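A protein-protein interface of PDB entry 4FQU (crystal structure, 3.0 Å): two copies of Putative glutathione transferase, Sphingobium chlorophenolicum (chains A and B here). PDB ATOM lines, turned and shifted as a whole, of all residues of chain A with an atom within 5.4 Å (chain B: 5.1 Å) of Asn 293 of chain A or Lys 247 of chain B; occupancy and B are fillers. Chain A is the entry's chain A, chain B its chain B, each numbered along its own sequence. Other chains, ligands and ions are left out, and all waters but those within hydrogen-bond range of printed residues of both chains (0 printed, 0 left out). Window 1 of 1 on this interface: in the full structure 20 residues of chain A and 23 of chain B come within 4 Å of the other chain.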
ATOM      1  N   HIS A 245       4.511  16.438  -1.290  1.00  0.00           N
ATOM      2  CA  HIS A 245       5.767  16.296  -0.570  1.00  0.00           C
ATOM      3  C   HIS A 245       6.542  15.048  -0.980  1.00  0.00           C
ATOM      4  O   HIS A 245       7.711  15.125  -1.386  1.00  0.00           O
ATOM      5  CB  HIS A 245       5.434  16.305   0.918  1.00  0.00           C
ATOM      6  CG  HIS A 245       6.602  16.417   1.834  1.00  0.00           C
ATOM      7  ND1 HIS A 245       6.847  15.487   2.821  1.00  0.00           N
ATOM      8  CD2 HIS A 245       7.528  17.386   1.987  1.00  0.00           C
ATOM      9  CE1 HIS A 245       7.912  15.846   3.512  1.00  0.00           C
ATOM     10  NE2 HIS A 245       8.349  16.990   3.021  1.00  0.00           N
ATOM     11  N   TYR A 286       5.614  18.852   6.046  1.00  0.00           N
ATOM     12  CA  TYR A 286       6.325  19.889   5.324  1.00  0.00           C
ATOM     13  C   TYR A 286       7.421  20.604   6.155  1.00  0.00           C
ATOM     14  O   TYR A 286       8.315  21.287   5.607  1.00  0.00           O
ATOM     15  CB  TYR A 286       5.332  20.875   4.788  1.00  0.00           C
ATOM     16  CG  TYR A 286       4.674  20.388   3.577  1.00  0.00           C
ATOM     17  CD1 TYR A 286       5.288  20.495   2.370  1.00  0.00           C
ATOM     18  CD2 TYR A 286       3.446  19.819   3.625  1.00  0.00           C
ATOM     19  CE1 TYR A 286       4.694  20.069   1.204  1.00  0.00           C
ATOM     20  CE2 TYR A 286       2.813  19.378   2.465  1.00  0.00           C
ATOM     21  CZ  TYR A 286       3.453  19.505   1.237  1.00  0.00           C
ATOM     22  OH  TYR A 286       2.872  19.080   0.044  1.00  0.00           O
ATOM     23  N   GLY A 287       7.369  20.432   7.466  1.00  0.00           N
ATOM     24  CA  GLY A 287       8.095  21.332   8.326  1.00  0.00           C
ATOM     25  C   GLY A 287       9.172  20.598   9.035  1.00  0.00           C
ATOM     26  O   GLY A 287       9.982  21.229   9.716  1.00  0.00           O
ATOM     27  N   HIS A 289      11.028  17.788   7.400  1.00  0.00           N
ATOM     28  CA  HIS A 289      11.826  17.016   6.448  1.00  0.00           C
ATOM     29  C   HIS A 289      12.653  17.961   5.592  1.00  0.00           C
ATOM     30  O   HIS A 289      12.276  18.265   4.465  1.00  0.00           O
ATOM     31  CB  HIS A 289      10.910  16.275   5.475  1.00  0.00           C
ATOM     32  CG  HIS A 289      10.121  15.172   6.079  1.00  0.00           C
ATOM     33  ND1 HIS A 289      10.315  14.728   7.370  1.00  0.00           N
ATOM     34  CD2 HIS A 289       9.133  14.404   5.562  1.00  0.00           C
ATOM     35  CE1 HIS A 289       9.480  13.739   7.624  1.00  0.00           C
ATOM     36  NE2 HIS A 289       8.747  13.525   6.544  1.00  0.00           N
ATOM     37  N   PRO A 290      13.794  18.413   6.086  1.00  0.00           N
ATOM     38  CA  PRO A 290      14.475  19.400   5.252  1.00  0.00           C
ATOM     39  C   PRO A 290      15.251  18.780   4.058  1.00  0.00           C
ATOM     40  O   PRO A 290      15.374  19.453   3.046  1.00  0.00           O
ATOM     41  CB  PRO A 290      15.382  20.107   6.249  1.00  0.00           C
ATOM     42  CG  PRO A 290      15.254  19.323   7.547  1.00  0.00           C
ATOM     43  CD  PRO A 290      14.598  18.040   7.237  1.00  0.00           C
ATOM     44  N   SER A 291      15.762  17.556   4.179  1.00  0.00           N
ATOM     45  CA  SER A 291      16.223  16.744   3.055  1.00  0.00           C
ATOM     46  C   SER A 291      15.314  16.889   1.842  1.00  0.00           C
ATOM     47  O   SER A 291      15.791  16.972   0.710  1.00  0.00           O
ATOM     48  CB  SER A 291      16.224  15.257   3.447  1.00  0.00           C
ATOM     49  OG  SER A 291      15.366  15.026   4.599  1.00  0.00           O
ATOM     50  N   VAL A 292      14.006  16.897   2.067  1.00  0.00           N
ATOM     51  CA  VAL A 292      13.040  16.890   0.983  1.00  0.00           C
ATOM     52  C   VAL A 292      12.470  18.282   0.739  1.00  0.00           C
ATOM     53  O   VAL A 292      12.243  18.660  -0.412  1.00  0.00           O
ATOM     54  CB  VAL A 292      11.861  15.986   1.328  1.00  0.00           C
ATOM     55  CG1 VAL A 292      10.878  15.937   0.221  1.00  0.00           C
ATOM     56  CG2 VAL A 292      12.343  14.608   1.652  1.00  0.00           C
ATOM     57  N   ASN A 293      12.229  19.035   1.819  1.00  0.00           N
ATOM     58  CA  ASN A 293      11.566  20.358   1.763  1.00  0.00           C
ATOM     59  C   ASN A 293      12.220  21.353   2.705  1.00  0.00           C
ATOM     60  O   ASN A 293      11.701  21.623   3.809  1.00  0.00           O
ATOM     61  CB  ASN A 293      10.052  20.266   2.071  1.00  0.00           C
ATOM     62  CG  ASN A 293       9.359  21.593   1.981  1.00  0.00           C
ATOM     63  OD1 ASN A 293       9.744  22.431   1.182  1.00  0.00           O
ATOM     64  ND2 ASN A 293       8.370  21.818   2.831  1.00  0.00           N
ATOM     65  N   PRO A 294      13.350  21.913   2.249  1.00  0.00           N
ATOM     66  CA  PRO A 294      14.243  22.804   2.988  1.00  0.00           C
ATOM     67  C   PRO A 294      13.547  24.083   3.462  1.00  0.00           C
ATOM     68  O   PRO A 294      13.919  24.508   4.545  1.00  0.00           O
ATOM     69  CB  PRO A 294      15.310  23.171   1.962  1.00  0.00           C
ATOM     70  CG  PRO A 294      15.103  22.279   0.810  1.00  0.00           C
ATOM     71  CD  PRO A 294      13.686  21.874   0.816  1.00  0.00           C
ATOM     72  N   THR A 295      12.620  24.719   2.737  1.00  0.00           N
ATOM     73  CA  THR A 295      12.144  25.986   3.316  1.00  0.00           C
ATOM     74  C   THR A 295      11.291  25.718   4.546  1.00  0.00           C
ATOM     75  O   THR A 295      11.095  26.608   5.385  1.00  0.00           O
ATOM     76  CB  THR A 295      11.371  26.897   2.351  1.00  0.00           C
ATOM     77  OG1 THR A 295      10.215  26.223   1.837  1.00  0.00           O
ATOM     78  CG2 THR A 295      12.227  27.279   1.223  1.00  0.00           C
ATOM     79  N   GLY A 296      10.794  24.481   4.643  1.00  0.00           N
ATOM     80  CA  GLY A 296       9.851  24.087   5.683  1.00  0.00           C
ATOM     81  C   GLY A 296       8.459  24.660   5.511  1.00  0.00           C
ATOM     82  O   GLY A 296       7.605  24.471   6.351  1.00  0.00           O
ATOM     83  N   ILE A 297       8.256  25.381   4.415  1.00  0.00           N
ATOM     84  CA  ILE A 297       7.012  26.072   4.120  1.00  0.00           C
ATOM     85  C   ILE A 297       5.907  25.087   3.782  1.00  0.00           C
ATOM     86  O   ILE A 297       6.125  24.143   3.017  1.00  0.00           O
ATOM     87  CB  ILE A 297       7.157  26.969   2.897  1.00  0.00           C
ATOM     88  CG1 ILE A 297       7.940  28.230   3.249  1.00  0.00           C
ATOM     89  CG2 ILE A 297       5.782  27.235   2.282  1.00  0.00           C
ATOM     90  CD1 ILE A 297       8.480  28.906   2.046  1.00  0.00           C
ATOM     91  N   VAL A 298       4.720  25.321   4.340  1.00  0.00           N
ATOM     92  CA  VAL A 298       3.605  24.417   4.173  1.00  0.00           C
ATOM     93  C   VAL A 298       2.700  24.904   3.062  1.00  0.00           C
ATOM     94  O   VAL A 298       2.211  26.006   3.161  1.00  0.00           O
ATOM     95  CB  VAL A 298       2.819  24.361   5.448  1.00  0.00           C
ATOM     96  CG1 VAL A 298       1.594  23.488   5.267  1.00  0.00           C
ATOM     97  CG2 VAL A 298       3.713  23.797   6.554  1.00  0.00           C
ATOM     98  N   PRO A 299       2.463  24.076   2.003  1.00  0.00           N
ATOM     99  CA  PRO A 299       1.716  24.599   0.863  1.00  0.00           C
ATOM    100  C   PRO A 299       0.408  25.020   1.377  1.00  0.00           C
ATOM    101  O   PRO A 299      -0.128  24.422   2.332  1.00  0.00           O
ATOM    102  CB  PRO A 299       1.505  23.382  -0.023  1.00  0.00           C
ATOM    103  CG  PRO A 299       2.435  22.400   0.425  1.00  0.00           C
ATOM    104  CD  PRO A 299       2.705  22.626   1.858  1.00  0.00           C
ATOM    105  N   VAL A 300      -0.118  26.056   0.747  1.00  0.00           N
ATOM    106  CA  VAL A 300      -1.470  26.512   1.018  1.00  0.00           C
ATOM    107  C   VAL A 300      -2.436  25.346   0.869  1.00  0.00           C
ATOM    108  O   VAL A 300      -3.646  25.494   0.952  1.00  0.00           O
ATOM    109  CB  VAL A 300      -1.803  27.648   0.081  1.00  0.00           C
ATOM    110  CG1 VAL A 300      -2.653  27.171  -1.138  1.00  0.00           C
ATOM    111  CG2 VAL A 300      -2.431  28.725   0.873  1.00  0.00           C
ATOM    112  N   TYR B 195       5.482  33.441   0.938  1.00  0.00           N
ATOM    113  CA  TYR B 195       4.865  32.474   0.085  1.00  0.00           C
ATOM    114  C   TYR B 195       3.423  32.900  -0.085  1.00  0.00           C
ATOM    115  O   TYR B 195       2.969  33.123  -1.205  1.00  0.00           O
ATOM    116  CB  TYR B 195       5.004  31.070   0.709  1.00  0.00           C
ATOM    117  CG  TYR B 195       4.028  30.040   0.184  1.00  0.00           C
ATOM    118  CD1 TYR B 195       3.848  29.840  -1.173  1.00  0.00           C
ATOM    119  CD2 TYR B 195       3.293  29.256   1.047  1.00  0.00           C
ATOM    120  CE1 TYR B 195       2.957  28.881  -1.655  1.00  0.00           C
ATOM    121  CE2 TYR B 195       2.377  28.304   0.569  1.00  0.00           C
ATOM    122  CZ  TYR B 195       2.226  28.129  -0.774  1.00  0.00           C
ATOM    123  OH  TYR B 195       1.353  27.186  -1.223  1.00  0.00           O
ATOM    124  N   PHE B 199       0.713  33.971  -3.960  1.00  0.00           N
ATOM    125  CA  PHE B 199      -0.094  33.146  -4.826  1.00  0.00           C
ATOM    126  C   PHE B 199      -1.574  33.029  -4.450  1.00  0.00           C
ATOM    127  O   PHE B 199      -2.400  32.614  -5.284  1.00  0.00           O
ATOM    128  CB  PHE B 199       0.487  31.782  -4.774  1.00  0.00           C
ATOM    129  CG  PHE B 199       0.195  31.140  -3.533  1.00  0.00           C
ATOM    130  CD1 PHE B 199      -0.127  29.815  -3.483  1.00  0.00           C
ATOM    131  CD2 PHE B 199       0.190  31.886  -2.406  1.00  0.00           C
ATOM    132  CE1 PHE B 199      -0.418  29.216  -2.292  1.00  0.00           C
ATOM    133  CE2 PHE B 199      -0.114  31.326  -1.221  1.00  0.00           C
ATOM    134  CZ  PHE B 199      -0.412  29.966  -1.151  1.00  0.00           C
ATOM    135  N   TYR B 242       4.433  23.626 -11.570  1.00  0.00           N
ATOM    136  CA  TYR B 242       4.136  24.672 -10.593  1.00  0.00           C
ATOM    137  C   TYR B 242       3.326  24.193  -9.409  1.00  0.00           C
ATOM    138  O   TYR B 242       3.634  24.477  -8.248  1.00  0.00           O
ATOM    139  CB  TYR B 242       3.396  25.793 -11.286  1.00  0.00           C
ATOM    140  CG  TYR B 242       4.190  26.459 -12.400  1.00  0.00           C
ATOM    141  CD1 TYR B 242       5.556  26.580 -12.318  1.00  0.00           C
ATOM    142  CD2 TYR B 242       3.560  26.959 -13.542  1.00  0.00           C
ATOM    143  CE1 TYR B 242       6.276  27.175 -13.311  1.00  0.00           C
ATOM    144  CE2 TYR B 242       4.288  27.552 -14.543  1.00  0.00           C
ATOM    145  CZ  TYR B 242       5.649  27.661 -14.411  1.00  0.00           C
ATOM    146  OH  TYR B 242       6.402  28.269 -15.385  1.00  0.00           O
ATOM    147  N   HIS B 243       2.256  23.473  -9.713  1.00  0.00           N
ATOM    148  CA  HIS B 243       1.396  22.909  -8.671  1.00  0.00           C
ATOM    149  C   HIS B 243       2.228  22.145  -7.652  1.00  0.00           C
ATOM    150  O   HIS B 243       2.136  22.400  -6.475  1.00  0.00           O
ATOM    151  CB  HIS B 243       0.341  22.014  -9.311  1.00  0.00           C
ATOM    152  CG  HIS B 243      -0.652  21.455  -8.351  1.00  0.00           C
ATOM    153  ND1 HIS B 243      -0.374  20.378  -7.542  1.00  0.00           N
ATOM    154  CD2 HIS B 243      -1.936  21.807  -8.097  1.00  0.00           C
ATOM    155  CE1 HIS B 243      -1.446  20.094  -6.826  1.00  0.00           C
ATOM    156  NE2 HIS B 243      -2.411  20.940  -7.149  1.00  0.00           N
ATOM    157  N   GLY B 244       3.068  21.230  -8.120  1.00  0.00           N
ATOM    158  CA  GLY B 244       3.982  20.524  -7.237  1.00  0.00           C
ATOM    159  C   GLY B 244       5.154  21.316  -6.647  1.00  0.00           C
ATOM    160  O   GLY B 244       5.245  21.538  -5.444  1.00  0.00           O
ATOM    161  N   HIS B 245       6.023  21.782  -7.524  1.00  0.00           N
ATOM    162  CA  HIS B 245       7.378  22.198  -7.210  1.00  0.00           C
ATOM    163  C   HIS B 245       7.370  23.543  -6.596  1.00  0.00           C
ATOM    164  O   HIS B 245       8.148  23.800  -5.705  1.00  0.00           O
ATOM    165  CB  HIS B 245       8.154  22.240  -8.520  1.00  0.00           C
ATOM    166  CG  HIS B 245       9.579  22.669  -8.398  1.00  0.00           C
ATOM    167  ND1 HIS B 245      10.130  23.641  -9.214  1.00  0.00           N
ATOM    168  CD2 HIS B 245      10.586  22.209  -7.622  1.00  0.00           C
ATOM    169  CE1 HIS B 245      11.404  23.795  -8.913  1.00  0.00           C
ATOM    170  NE2 HIS B 245      11.706  22.941  -7.949  1.00  0.00           N
ATOM    171  N   PHE B 246       6.488  24.410  -7.078  1.00  0.00           N
ATOM    172  CA  PHE B 246       6.323  25.763  -6.520  1.00  0.00           C
ATOM    173  C   PHE B 246       5.118  25.894  -5.534  1.00  0.00           C
ATOM    174  O   PHE B 246       4.649  27.010  -5.305  1.00  0.00           O
ATOM    175  CB  PHE B 246       6.165  26.813  -7.638  1.00  0.00           C
ATOM    176  CG  PHE B 246       7.415  27.116  -8.403  1.00  0.00           C
ATOM    177  CD1 PHE B 246       8.639  26.708  -7.976  1.00  0.00           C
ATOM    178  CD2 PHE B 246       7.358  27.851  -9.553  1.00  0.00           C
ATOM    179  CE1 PHE B 246       9.776  27.025  -8.689  1.00  0.00           C
ATOM    180  CE2 PHE B 246       8.504  28.151 -10.249  1.00  0.00           C
ATOM    181  CZ  PHE B 246       9.699  27.728  -9.808  1.00  0.00           C
ATOM    182  N   LYS B 247       4.610  24.786  -4.976  1.00  0.00           N
ATOM    183  CA  LYS B 247       3.515  24.853  -4.009  1.00  0.00           C
ATOM    184  C   LYS B 247       2.301  25.722  -4.434  1.00  0.00           C
ATOM    185  O   LYS B 247       1.612  26.351  -3.593  1.00  0.00           O
ATOM    186  CB  LYS B 247       4.050  25.354  -2.683  1.00  0.00           C
ATOM    187  CG  LYS B 247       4.891  24.366  -2.026  1.00  0.00           C
ATOM    188  CD  LYS B 247       5.542  24.907  -0.763  1.00  0.00           C
ATOM    189  CE  LYS B 247       6.542  23.913  -0.156  1.00  0.00           C
ATOM    190  NZ  LYS B 247       7.705  23.632  -1.078  1.00  0.00           N
ATOM    191  N   CYS B 248       2.036  25.753  -5.735  1.00  0.00           N
ATOM    192  CA  CYS B 248       0.954  26.556  -6.209  1.00  0.00           C
ATOM    193  C   CYS B 248      -0.300  25.688  -6.239  1.00  0.00           C
ATOM    194  O   CYS B 248      -0.927  25.532  -7.291  1.00  0.00           O
ATOM    195  CB  CYS B 248       1.334  27.070  -7.579  1.00  0.00           C
ATOM    196  SG  CYS B 248       2.397  28.538  -7.487  1.00  0.00           S
ATOM    197  N   ASN B 249      -0.676  25.120  -5.091  1.00  0.00           N
ATOM    198  CA  ASN B 249      -1.515  23.919  -5.133  1.00  0.00           C
ATOM    199  C   ASN B 249      -2.956  24.066  -4.635  1.00  0.00           C
ATOM    200  O   ASN B 249      -3.703  23.090  -4.520  1.00  0.00           O
ATOM    201  CB  ASN B 249      -0.822  22.765  -4.403  1.00  0.00           C
ATOM    202  CG  ASN B 249      -0.949  22.882  -2.905  1.00  0.00           C
ATOM    203  OD1 ASN B 249      -1.224  23.976  -2.428  1.00  0.00           O
ATOM    204  ND2 ASN B 249      -0.755  21.770  -2.151  1.00  0.00           N
ATOM    205  N   VAL B 292      14.975  24.637  -3.782  1.00  0.00           N
ATOM    206  CA  VAL B 292      13.544  24.369  -3.686  1.00  0.00           C
ATOM    207  C   VAL B 292      13.313  22.880  -3.588  1.00  0.00           C
ATOM    208  O   VAL B 292      12.480  22.429  -2.799  1.00  0.00           O
ATOM    209  CB  VAL B 292      12.824  24.843  -4.950  1.00  0.00           C
ATOM    210  CG1 VAL B 292      11.511  24.180  -5.083  1.00  0.00           C
ATOM    211  CG2 VAL B 292      12.657  26.336  -4.945  1.00  0.00           C
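Val 292 of chain B touches Pro 294 of chain A (O to CD, 3.9 Å).
Ile 297 of chain A touches Tyr 195 of chain B.
Lys 247 of chain B touches Ile 297 of chain A (CE to O, 3.2 Å).
Val 298 of chain A touches Tyr 195 of chain B (O to CE2, 3.5 Å).
Pro 299 of chain A touches Tyr 195 of chain B.
Pro 299 of chain A touches Lys 247 of chain B.
Asn 249 of chain B touches Pro 299 of chain A.
Val 300 of chain A touches Phe 199 of chain B (CB to CZ, 3.0 Å).
OD1 of Asn 249 of chain B touches CG1 of Val 300 of chain A, 3.7 Å away.
O of Tyr 286 of chain A sits at hydrogen-bond distance from ND2 of Asn 293 of chain A (2.8 Å).
The side-chain amide nitrogen of Asn 293 of chain A is in hydrogen-bond range of the backbone carbonyl oxygen of Ile 297 of chain A.
The backbone NH (N) of Ile 297 of chain A sits close to the side-chain hydroxyl (OG1) of Thr 295 of chain A (3.3 Å).
The backbone carbonyl oxygen of Lys 247 of chain B is in hydrogen-bond range of the side-chain hydroxyl of Tyr 195 of chain B (2.5 Å).
The backbone carbonyl oxygen (O) of Tyr 242 of chain B sits at hydrogen-bond distance from the backbone NH (N) of Lys 247 of chain B (3.4 Å).
The side-chain amino group (NZ) of Lys 247 of chain B is in hydrogen-bond range of the side-chain amide oxygen (OD1) of Asn 293 of chain A, at 3.3 Å.
N of Val 300 of chain A lies within hydrogen-bond range of OH of Tyr 195 of chain B.
Asn 293 of chain A touches just one residue of chain B: Lys 247 (3.3 Å).
Gly 296 of chain A touches none of the printed residues of chain B.
Printed residues of chain B within 4 Å of Ile 297 of chain A: Tyr 195 and Lys 247.
Printed residues of chain B within 4 Å of Val 300 of chain A: Tyr 195, Phe 199 and Asn 249.
Printed residues of chain A within 4 Å of Lys 247 of chain B: Asn 293, Ile 297 and Pro 299.
The nearest printed residue of chain A that does not touch Lys 247 of chain B is Tyr 286 of chain A (4.4 Å).
The nearest printed residue of chain B that does not touch Pro 299 of chain A is Phe 199 of chain B (5.6 Å).
Hydrophobic or aromatic side chains of chain B within 4 Å of the printed part of chain A: Tyr 195 and Phe 199.
Of the 15 printed residues of chain A, 6 touch a printed residue of chain B.
Hydrophobic or aromatic side chains of chain A that line the printed part of chain B: Pro 294, Ile 297, Pro 299 and Val 300.
Among the printed residues, no Asp or Glu carboxylate lies within 4 Å of a Lys or Arg side-chain nitrogen of the other chain.
Positions printed for both chains: 245 and 292.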
